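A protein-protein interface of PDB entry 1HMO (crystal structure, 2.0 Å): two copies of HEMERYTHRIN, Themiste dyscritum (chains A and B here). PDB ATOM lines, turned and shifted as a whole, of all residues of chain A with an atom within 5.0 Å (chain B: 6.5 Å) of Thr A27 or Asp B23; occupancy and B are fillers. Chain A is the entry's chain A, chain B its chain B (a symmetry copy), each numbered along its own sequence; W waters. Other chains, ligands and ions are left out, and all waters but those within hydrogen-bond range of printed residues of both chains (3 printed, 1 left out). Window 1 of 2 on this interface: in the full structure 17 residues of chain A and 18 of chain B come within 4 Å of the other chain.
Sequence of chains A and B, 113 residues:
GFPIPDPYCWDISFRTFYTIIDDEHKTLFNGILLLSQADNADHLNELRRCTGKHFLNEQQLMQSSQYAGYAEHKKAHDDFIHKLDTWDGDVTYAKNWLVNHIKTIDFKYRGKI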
ATOM      1  N   ASP A  23       9.936  -8.546 -26.030  1.00  0.00           N
ATOM      2  CA  ASP A  23       8.871  -8.135 -25.050  1.00  0.00           C
ATOM      3  C   ASP A  23       9.469  -7.344 -23.937  1.00  0.00           C
ATOM      4  O   ASP A  23       8.876  -6.323 -23.511  1.00  0.00           O
ATOM      5  CB  ASP A  23       8.078  -9.362 -24.630  1.00  0.00           C
ATOM      6  CG  ASP A  23       7.211  -9.883 -25.723  1.00  0.00           C
ATOM      7  OD1 ASP A  23       6.649 -10.978 -25.618  1.00  0.00           O
ATOM      8  OD2 ASP A  23       6.997  -9.164 -26.740  1.00  0.00           O
ATOM      9  N   GLU A  24      10.642  -7.717 -23.449  1.00  0.00           N
ATOM     10  CA  GLU A  24      11.269  -6.901 -22.391  1.00  0.00           C
ATOM     11  C   GLU A  24      11.652  -5.546 -22.875  1.00  0.00           C
ATOM     12  O   GLU A  24      11.461  -4.530 -22.170  1.00  0.00           O
ATOM     13  CB  GLU A  24      12.542  -7.611 -21.838  1.00  0.00           C
ATOM     14  CG  GLU A  24      12.212  -8.863 -21.031  1.00  0.00           C
ATOM     15  CD  GLU A  24      13.297  -9.651 -20.369  1.00  0.00           C
ATOM     16  OE1 GLU A  24      12.981 -10.501 -19.528  1.00  0.00           O
ATOM     17  OE2 GLU A  24      14.465  -9.398 -20.708  1.00  0.00           O
ATOM     18  N   HIS A  25      12.207  -5.492 -24.097  1.00  0.00           N
ATOM     19  CA  HIS A  25      12.618  -4.176 -24.654  1.00  0.00           C
ATOM     20  C   HIS A  25      11.459  -3.196 -24.697  1.00  0.00           C
ATOM     21  O   HIS A  25      11.623  -1.994 -24.394  1.00  0.00           O
ATOM     22  CB  HIS A  25      13.267  -4.299 -26.045  1.00  0.00           C
ATOM     23  CG  HIS A  25      14.667  -4.858 -25.976  1.00  0.00           C
ATOM     24  ND1 HIS A  25      15.275  -5.466 -27.068  1.00  0.00           N
ATOM     25  CD2 HIS A  25      15.557  -4.930 -24.971  1.00  0.00           C
ATOM     26  CE1 HIS A  25      16.511  -5.755 -26.711  1.00  0.00           C
ATOM     27  NE2 HIS A  25      16.728  -5.501 -25.433  1.00  0.00           N
ATOM     28  N   LYS A  26      10.311  -3.691 -25.082  1.00  0.00           N
ATOM     29  CA  LYS A  26       9.082  -2.881 -25.118  1.00  0.00           C
ATOM     30  C   LYS A  26       8.850  -2.235 -23.778  1.00  0.00           C
ATOM     31  O   LYS A  26       8.388  -1.089 -23.669  1.00  0.00           O
ATOM     32  CB  LYS A  26       7.911  -3.749 -25.515  1.00  0.00           C
ATOM     33  CG  LYS A  26       7.928  -4.202 -26.973  1.00  0.00           C
ATOM     34  CD  LYS A  26       6.870  -5.256 -27.239  1.00  0.00           C
ATOM     35  CE  LYS A  26       7.219  -6.021 -28.521  1.00  0.00           C
ATOM     36  NZ  LYS A  26       6.356  -7.163 -28.709  1.00  0.00           N
ATOM     37  N   THR A  27       9.184  -2.910 -22.694  1.00  0.00           N
ATOM     38  CA  THR A  27       8.969  -2.334 -21.378  1.00  0.00           C
ATOM     39  C   THR A  27       9.978  -1.239 -21.163  1.00  0.00           C
ATOM     40  O   THR A  27       9.649  -0.299 -20.416  1.00  0.00           O
ATOM     41  CB  THR A  27       8.960  -3.384 -20.194  1.00  0.00           C
ATOM     42  OG1 THR A  27      10.352  -3.828 -19.939  1.00  0.00           O
ATOM     43  CG2 THR A  27       8.068  -4.585 -20.433  1.00  0.00           C
ATOM     44  N   LEU A  28      11.148  -1.298 -21.787  1.00  0.00           N
ATOM     45  CA  LEU A  28      12.148  -0.236 -21.509  1.00  0.00           C
ATOM     46  C   LEU A  28      11.729   1.018 -22.278  1.00  0.00           C
ATOM     47  O   LEU A  28      11.886   2.116 -21.699  1.00  0.00           O
ATOM     48  CB  LEU A  28      13.527  -0.741 -21.774  1.00  0.00           C
ATOM     49  CG  LEU A  28      14.026  -2.012 -21.115  1.00  0.00           C
ATOM     50  CD1 LEU A  28      15.556  -2.042 -21.304  1.00  0.00           C
ATOM     51  CD2 LEU A  28      13.753  -2.010 -19.652  1.00  0.00           C
ATOM     52  N   PHE A  29      11.247   0.868 -23.482  1.00  0.00           N
ATOM     53  CA  PHE A  29      10.740   2.056 -24.229  1.00  0.00           C
ATOM     54  C   PHE A  29       9.651   2.772 -23.420  1.00  0.00           C
ATOM     55  O   PHE A  29       9.640   4.016 -23.265  1.00  0.00           O
ATOM     56  CB  PHE A  29      10.237   1.621 -25.612  1.00  0.00           C
ATOM     57  CG  PHE A  29      11.349   1.481 -26.620  1.00  0.00           C
ATOM     58  CD1 PHE A  29      12.020   0.265 -26.754  1.00  0.00           C
ATOM     59  CD2 PHE A  29      11.670   2.583 -27.428  1.00  0.00           C
ATOM     60  CE1 PHE A  29      12.998   0.129 -27.746  1.00  0.00           C
ATOM     61  CE2 PHE A  29      12.707   2.503 -28.358  1.00  0.00           C
ATOM     62  CZ  PHE A  29      13.343   1.250 -28.495  1.00  0.00           C
ATOM     63  N   ASN A  30       8.701   1.987 -22.950  1.00  0.00           N
ATOM     64  CA  ASN A  30       7.584   2.519 -22.137  1.00  0.00           C
ATOM     65  C   ASN A  30       8.085   3.269 -20.912  1.00  0.00           C
ATOM     66  O   ASN A  30       7.547   4.350 -20.610  1.00  0.00           O
ATOM     67  CB  ASN A  30       6.593   1.406 -21.767  1.00  0.00           C
ATOM     68  CG  ASN A  30       5.440   1.910 -20.894  1.00  0.00           C
ATOM     69  OD1 ASN A  30       4.509   2.524 -21.425  1.00  0.00           O
ATOM     70  ND2 ASN A  30       5.600   1.785 -19.574  1.00  0.00           N
ATOM     71  N   GLY A  31       9.038   2.744 -20.184  1.00  0.00           N
ATOM     72  CA  GLY A  31       9.626   3.349 -19.005  1.00  0.00           C
ATOM     73  C   GLY A  31      10.217   4.726 -19.337  1.00  0.00           C
ATOM     74  O   GLY A  31      10.033   5.643 -18.542  1.00  0.00           O
ATOM     75  N   GLU A  46       9.554   2.282 -12.126  1.00  0.00           N
ATOM     76  CA  GLU A  46       9.101   1.380 -13.170  1.00  0.00           C
ATOM     77  C   GLU A  46      10.212   1.038 -14.168  1.00  0.00           C
ATOM     78  O   GLU A  46      10.494  -0.108 -14.569  1.00  0.00           O
ATOM     79  CB  GLU A  46       7.922   2.015 -13.897  1.00  0.00           C
ATOM     80  CG  GLU A  46       6.920   1.092 -14.540  1.00  0.00           C
ATOM     81  CD  GLU A  46       6.243   0.024 -13.771  1.00  0.00           C
ATOM     82  OE1 GLU A  46       5.868  -1.036 -14.243  1.00  0.00           O
ATOM     83  OE2 GLU A  46       5.976   0.328 -12.573  1.00  0.00           O
ATOM     84  N   ARG A  49      13.102  -0.885 -12.403  1.00  0.00           N
ATOM     85  CA  ARG A  49      12.754  -2.310 -12.183  1.00  0.00           C
ATOM     86  C   ARG A  49      12.882  -3.037 -13.520  1.00  0.00           C
ATOM     87  O   ARG A  49      13.572  -4.083 -13.604  1.00  0.00           O
ATOM     88  CB  ARG A  49      11.381  -2.512 -11.577  1.00  0.00           C
ATOM     89  CG  ARG A  49      10.883  -3.929 -11.391  1.00  0.00           C
ATOM     90  CD  ARG A  49       9.457  -4.031 -11.033  1.00  0.00           C
ATOM     91  NE  ARG A  49       8.460  -3.580 -11.987  1.00  0.00           N
ATOM     92  CZ  ARG A  49       8.092  -4.194 -13.110  1.00  0.00           C
ATOM     93  NH1 ARG A  49       7.110  -3.743 -13.912  1.00  0.00           N
ATOM     94  NH2 ARG A  49       8.745  -5.298 -13.500  1.00  0.00           N
ATOM     95  N   CYS A  50      12.208  -2.573 -14.537  1.00  0.00           N
ATOM     96  CA  CYS A  50      12.265  -3.258 -15.855  1.00  0.00           C
ATOM     97  C   CYS A  50      13.642  -3.402 -16.428  1.00  0.00           C
ATOM     98  O   CYS A  50      13.966  -4.432 -17.061  1.00  0.00           O
ATOM     99  CB  CYS A  50      11.313  -2.526 -16.801  1.00  0.00           C
ATOM    100  SG  CYS A  50       9.631  -2.778 -16.333  1.00  0.00           S
ATOM    101  N   LYS A  53      15.794  -5.991 -14.380  1.00  0.00           N
ATOM    102  CA  LYS A  53      15.297  -7.325 -14.746  1.00  0.00           C
ATOM    103  C   LYS A  53      15.753  -7.706 -16.149  1.00  0.00           C
ATOM    104  O   LYS A  53      16.199  -8.865 -16.420  1.00  0.00           O
ATOM    105  CB  LYS A  53      13.788  -7.357 -14.676  1.00  0.00           C
ATOM    106  CG  LYS A  53      13.096  -8.661 -15.076  1.00  0.00           C
ATOM    107  CD  LYS A  53      11.553  -8.399 -15.057  1.00  0.00           C
ATOM    108  CE  LYS A  53      10.986  -8.528 -16.438  1.00  0.00           C
ATOM    109  NZ  LYS A  53      10.168  -7.403 -16.919  1.00  0.00           N
ATOM    110  N   TRP B  10       0.970   2.341 -22.315  1.00  0.00           N
ATOM    111  CA  TRP B  10       0.647   1.986 -20.927  1.00  0.00           C
ATOM    112  C   TRP B  10       0.993   3.111 -19.998  1.00  0.00           C
ATOM    113  O   TRP B  10       2.028   3.805 -20.180  1.00  0.00           O
ATOM    114  CB  TRP B  10       1.427   0.683 -20.643  1.00  0.00           C
ATOM    115  CG  TRP B  10       1.137   0.121 -19.281  1.00  0.00           C
ATOM    116  CD1 TRP B  10       0.200  -0.839 -19.010  1.00  0.00           C
ATOM    117  CD2 TRP B  10       1.799   0.435 -18.076  1.00  0.00           C
ATOM    118  NE1 TRP B  10       0.275  -1.164 -17.672  1.00  0.00           N
ATOM    119  CE2 TRP B  10       1.231  -0.407 -17.079  1.00  0.00           C
ATOM    120  CE3 TRP B  10       2.776   1.351 -17.707  1.00  0.00           C
ATOM    121  CZ2 TRP B  10       1.619  -0.344 -15.733  1.00  0.00           C
ATOM    122  CZ3 TRP B  10       3.184   1.400 -16.407  1.00  0.00           C
ATOM    123  CH2 TRP B  10       2.622   0.559 -15.430  1.00  0.00           C
ATOM    124  N   TYR B  18       0.709  -6.631 -10.048  1.00  0.00           N
ATOM    125  CA  TYR B  18       1.308  -7.944 -10.415  1.00  0.00           C
ATOM    126  C   TYR B  18       2.333  -7.542 -11.510  1.00  0.00           C
ATOM    127  O   TYR B  18       1.875  -7.289 -12.642  1.00  0.00           O
ATOM    128  CB  TYR B  18       0.248  -8.901 -10.889  1.00  0.00           C
ATOM    129  CG  TYR B  18      -0.814  -9.272  -9.874  1.00  0.00           C
ATOM    130  CD1 TYR B  18      -0.522 -10.290  -8.937  1.00  0.00           C
ATOM    131  CD2 TYR B  18      -2.027  -8.623  -9.760  1.00  0.00           C
ATOM    132  CE1 TYR B  18      -1.437 -10.666  -7.961  1.00  0.00           C
ATOM    133  CE2 TYR B  18      -2.972  -8.968  -8.786  1.00  0.00           C
ATOM    134  CZ  TYR B  18      -2.644  -9.969  -7.867  1.00  0.00           C
ATOM    135  OH  TYR B  18      -3.501 -10.287  -6.883  1.00  0.00           O
ATOM    136  N   THR B  19       3.597  -7.369 -11.198  1.00  0.00           N
ATOM    137  CA  THR B  19       4.602  -6.865 -12.160  1.00  0.00           C
ATOM    138  C   THR B  19       4.656  -7.656 -13.438  1.00  0.00           C
ATOM    139  O   THR B  19       4.770  -6.998 -14.513  1.00  0.00           O
ATOM    140  CB  THR B  19       6.058  -6.679 -11.557  1.00  0.00           C
ATOM    141  OG1 THR B  19       6.521  -8.005 -11.250  1.00  0.00           O
ATOM    142  CG2 THR B  19       6.127  -5.744 -10.362  1.00  0.00           C
ATOM    143  N   ILE B  20       4.523  -8.946 -13.413  1.00  0.00           N
ATOM    144  CA  ILE B  20       4.542  -9.783 -14.607  1.00  0.00           C
ATOM    145  C   ILE B  20       3.381  -9.396 -15.539  1.00  0.00           C
ATOM    146  O   ILE B  20       3.543  -9.380 -16.773  1.00  0.00           O
ATOM    147  CB  ILE B  20       4.497 -11.302 -14.242  1.00  0.00           C
ATOM    148  CG1 ILE B  20       4.362 -12.178 -15.511  1.00  0.00           C
ATOM    149  CG2 ILE B  20       3.308 -11.675 -13.282  1.00  0.00           C
ATOM    150  CD1 ILE B  20       5.660 -12.209 -16.379  1.00  0.00           C
ATOM    151  N   ILE B  21       2.215  -9.227 -14.930  1.00  0.00           N
ATOM    152  CA  ILE B  21       0.973  -8.846 -15.585  1.00  0.00           C
ATOM    153  C   ILE B  21       1.137  -7.458 -16.219  1.00  0.00           C
ATOM    154  O   ILE B  21       0.874  -7.243 -17.411  1.00  0.00           O
ATOM    155  CB  ILE B  21      -0.247  -8.907 -14.595  1.00  0.00           C
ATOM    156  CG1 ILE B  21      -0.526 -10.378 -14.159  1.00  0.00           C
ATOM    157  CG2 ILE B  21      -1.521  -8.249 -15.144  1.00  0.00           C
ATOM    158  CD1 ILE B  21      -1.082 -11.342 -15.192  1.00  0.00           C
ATOM    159  N   ASP B  22       1.582  -6.518 -15.398  1.00  0.00           N
ATOM    160  CA  ASP B  22       1.773  -5.161 -15.915  1.00  0.00           C
ATOM    161  C   ASP B  22       2.745  -5.199 -17.085  1.00  0.00           C
ATOM    162  O   ASP B  22       2.557  -4.366 -17.997  1.00  0.00           O
ATOM    163  CB  ASP B  22       2.258  -4.201 -14.816  1.00  0.00           C
ATOM    164  CG  ASP B  22       1.200  -3.934 -13.737  1.00  0.00           C
ATOM    165  OD1 ASP B  22       0.020  -4.136 -13.994  1.00  0.00           O
ATOM    166  OD2 ASP B  22       1.608  -3.455 -12.668  1.00  0.00           O
ATOM    167  N   ASP B  23       3.842  -5.935 -16.965  1.00  0.00           N
ATOM    168  CA  ASP B  23       4.860  -5.937 -18.074  1.00  0.00           C
ATOM    169  C   ASP B  23       4.253  -6.509 -19.338  1.00  0.00           C
ATOM    170  O   ASP B  23       4.519  -6.031 -20.447  1.00  0.00           O
ATOM    171  CB  ASP B  23       6.146  -6.586 -17.652  1.00  0.00           C
ATOM    172  CG  ASP B  23       7.012  -5.789 -16.749  1.00  0.00           C
ATOM    173  OD1 ASP B  23       7.978  -6.331 -16.181  1.00  0.00           O
ATOM    174  OD2 ASP B  23       6.706  -4.608 -16.507  1.00  0.00           O
ATOM    175  N   GLU B  24       3.504  -7.614 -19.220  1.00  0.00           N
ATOM    176  CA  GLU B  24       2.787  -8.112 -20.370  1.00  0.00           C
ATOM    177  C   GLU B  24       1.803  -7.106 -20.933  1.00  0.00           C
ATOM    178  O   GLU B  24       1.634  -7.030 -22.167  1.00  0.00           O
ATOM    179  CB  GLU B  24       1.990  -9.395 -20.025  1.00  0.00           C
ATOM    180  CG  GLU B  24       2.989 -10.552 -19.851  1.00  0.00           C
ATOM    181  CD  GLU B  24       2.410 -11.846 -19.405  1.00  0.00           C
ATOM    182  OE1 GLU B  24       3.115 -12.859 -19.329  1.00  0.00           O
ATOM    183  OE2 GLU B  24       1.193 -11.842 -19.120  1.00  0.00           O
ATOM    184  N   HIS B  25       1.066  -6.415 -20.064  1.00  0.00           N
ATOM    185  CA  HIS B  25       0.122  -5.366 -20.557  1.00  0.00           C
ATOM    186  C   HIS B  25       0.788  -4.337 -21.438  1.00  0.00           C
ATOM    187  O   HIS B  25       0.226  -3.925 -22.481  1.00  0.00           O
ATOM    188  CB  HIS B  25      -0.620  -4.667 -19.368  1.00  0.00           C
ATOM    189  CG  HIS B  25      -1.727  -5.539 -18.859  1.00  0.00           C
ATOM    190  ND1 HIS B  25      -2.277  -5.285 -17.610  1.00  0.00           N
ATOM    191  CD2 HIS B  25      -2.303  -6.652 -19.307  1.00  0.00           C
ATOM    192  CE1 HIS B  25      -3.260  -6.122 -17.437  1.00  0.00           C
ATOM    193  NE2 HIS B  25      -3.290  -7.017 -18.414  1.00  0.00           N
ATOM    194  N   LYS B  26       1.953  -3.872 -21.066  1.00  0.00           N
ATOM    195  CA  LYS B  26       2.762  -2.940 -21.832  1.00  0.00           C
ATOM    196  C   LYS B  26       2.929  -3.456 -23.246  1.00  0.00           C
ATOM    197  O   LYS B  26       2.851  -2.648 -24.209  1.00  0.00           O
ATOM    198  CB  LYS B  26       4.141  -2.695 -21.194  1.00  0.00           C
ATOM    199  CG  LYS B  26       4.004  -1.988 -19.857  1.00  0.00           C
ATOM    200  CD  LYS B  26       5.284  -1.976 -19.056  1.00  0.00           C
ATOM    201  CE  LYS B  26       5.012  -1.599 -17.595  1.00  0.00           C
ATOM    202  NZ  LYS B  26       6.307  -1.619 -16.846  1.00  0.00           N
ATOM    203  N   THR B  27       3.092  -4.772 -23.423  1.00  0.00           N
ATOM    204  CA  THR B  27       3.238  -5.259 -24.801  1.00  0.00           C
ATOM    205  C   THR B  27       1.954  -5.208 -25.595  1.00  0.00           C
ATOM    206  O   THR B  27       2.014  -5.112 -26.869  1.00  0.00           O
ATOM    207  CB  THR B  27       3.896  -6.703 -24.836  1.00  0.00           C
ATOM    208  OG1 THR B  27       2.838  -7.613 -24.462  1.00  0.00           O
ATOM    209  CG2 THR B  27       5.154  -6.762 -23.958  1.00  0.00           C
ATOM    210  N   LEU B  28       0.798  -5.295 -24.977  1.00  0.00           N
ATOM    211  CA  LEU B  28      -0.489  -5.227 -25.708  1.00  0.00           C
ATOM    212  C   LEU B  28      -0.680  -3.770 -26.174  1.00  0.00           C
ATOM    213  O   LEU B  28      -1.148  -3.534 -27.300  1.00  0.00           O
ATOM    214  CB  LEU B  28      -1.601  -5.816 -24.880  1.00  0.00           C
ATOM    215  CG  LEU B  28      -1.634  -7.144 -24.209  1.00  0.00           C
ATOM    216  CD1 LEU B  28      -2.976  -7.415 -23.515  1.00  0.00           C
ATOM    217  CD2 LEU B  28      -1.368  -8.248 -25.222  1.00  0.00           C
HETATM  218  O   HOH W   1       8.153  -9.057 -15.419  1.00  0.00           O
HETATM  219  O   HOH W   2       3.838  -5.462 -29.083  1.00  0.00           O
HETATM  220  O   HOH W   3       3.813  -1.693 -12.287  1.00  0.00           O
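Among the printed residues, merely in contact across the chains: Asp A23 with Thr B27 (3.8 Å), Lys A26 with Thr B27 (3.997 Å), Thr A27 with Asp B23 (3.8 Å), Asn A30 with Lys B26 (3.8 Å), Glu A46 with Trp B10 (3.8 Å), Arg A49 with Thr B19 (3.6 Å) and Arg A49 with Lys B26 (3.7 Å).
OD2 of Asp B23 is in salt-bridge range of NZ of Lys B26 (3.0 Å). The guanidinium group (NH1) of Arg A49 sits at hydrogen-bond distance from the side-chain sulfur (SG) of Cys A50, at 3.6 Å. OG1 of Thr B27 is in hydrogen-bond range of O of Glu B24. The backbone carbonyl oxygen (O) of Glu A46 is in hydrogen-bond range of the side-chain sulfur (SG) of Cys A50 (3.3 Å). The side-chain carboxylate of Asp A23 is in salt-bridge range of the side-chain amino group of Lys A26 (2.9 Å). The backbone carbonyl oxygen (O) of Glu A24 is in hydrogen-bond range of the side-chain hydroxyl (OG1) of Thr A27 (2.6 Å).
Of chain B, only Asp B23 comes within 4 Å of Thr A27. Of the printed residues of chain B, Cys A50 touches Asp B23 and Lys B26. Printed residues of chain B within 4 Å of Lys A53: Asp B23. Of the printed residues of chain A, Trp B10 touches Asn A30 and Glu A46. Printed residues of chain A within 4 Å of Thr B27: Asp A23 and Lys A26. The nearest residue of chain B that does not touch Thr A27 is Lys B26 (4.1 Å). The nearest printed residue of chain A that does not touch Asp B23 is Glu A46 (4.3 Å).
Of the 12 printed residues of chain B, 5 touch a printed residue of chain A. Printed residues of chain B that touch a printed residue of chain A: Trp B10, Thr B19, Asp B23, Lys B26 and Thr B27. Along chain B the printed residues that touch a printed residue of chain A span positions 10 to 27.
Water W1 bridges the side-chain carboxylate of Asp B23 (2.8 Å) and the side-chain amino group of Lys A53 (3.0 Å). Water W3 bridges the side-chain carboxylate (OD2) of Asp B22 (2.8 Å) and the side-chain carboxylate (OE1) of Glu A46 (2.9 Å). Water W2 lies within hydrogen-bond range of O of Thr B27 (2.9 Å) and NZ of Lys A26 (3.1 Å).
The backbone carbonyl oxygen (O) of Trp B10 sits close to the side-chain amide oxygen (OD1) of Asn A30, at 3.1 Å. SG of Cys A50 sits at hydrogen-bond distance from NZ of Lys B26 (3.6 Å). The side-chain amino group of Lys B26 lies within salt-bridge range of the side-chain carboxylate of Glu A46 (2.7 Å). NH1 of Arg A49 is in salt-bridge range of OD2 of Asp B23 (2.8 Å). NZ of Lys A53 lies within salt-bridge range of OD1 of Asp B23. The side-chain carboxylate (OD2) of Asp B23 lies within hydrogen-bond range of the side-chain sulfur (SG) of Cys A50 (3.5 Å).
Asp A23 touches Thr B27, and with the chains exchanged Thr A27 touches Asp B23. Lys A26 touches Thr B27, but with the chains exchanged Thr A27 does not touch Lys B26 (4.1 Å). Of the 13 pairs that touch across the chains among the printed residues, 2 have their exchanged pair printed and touching as well.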
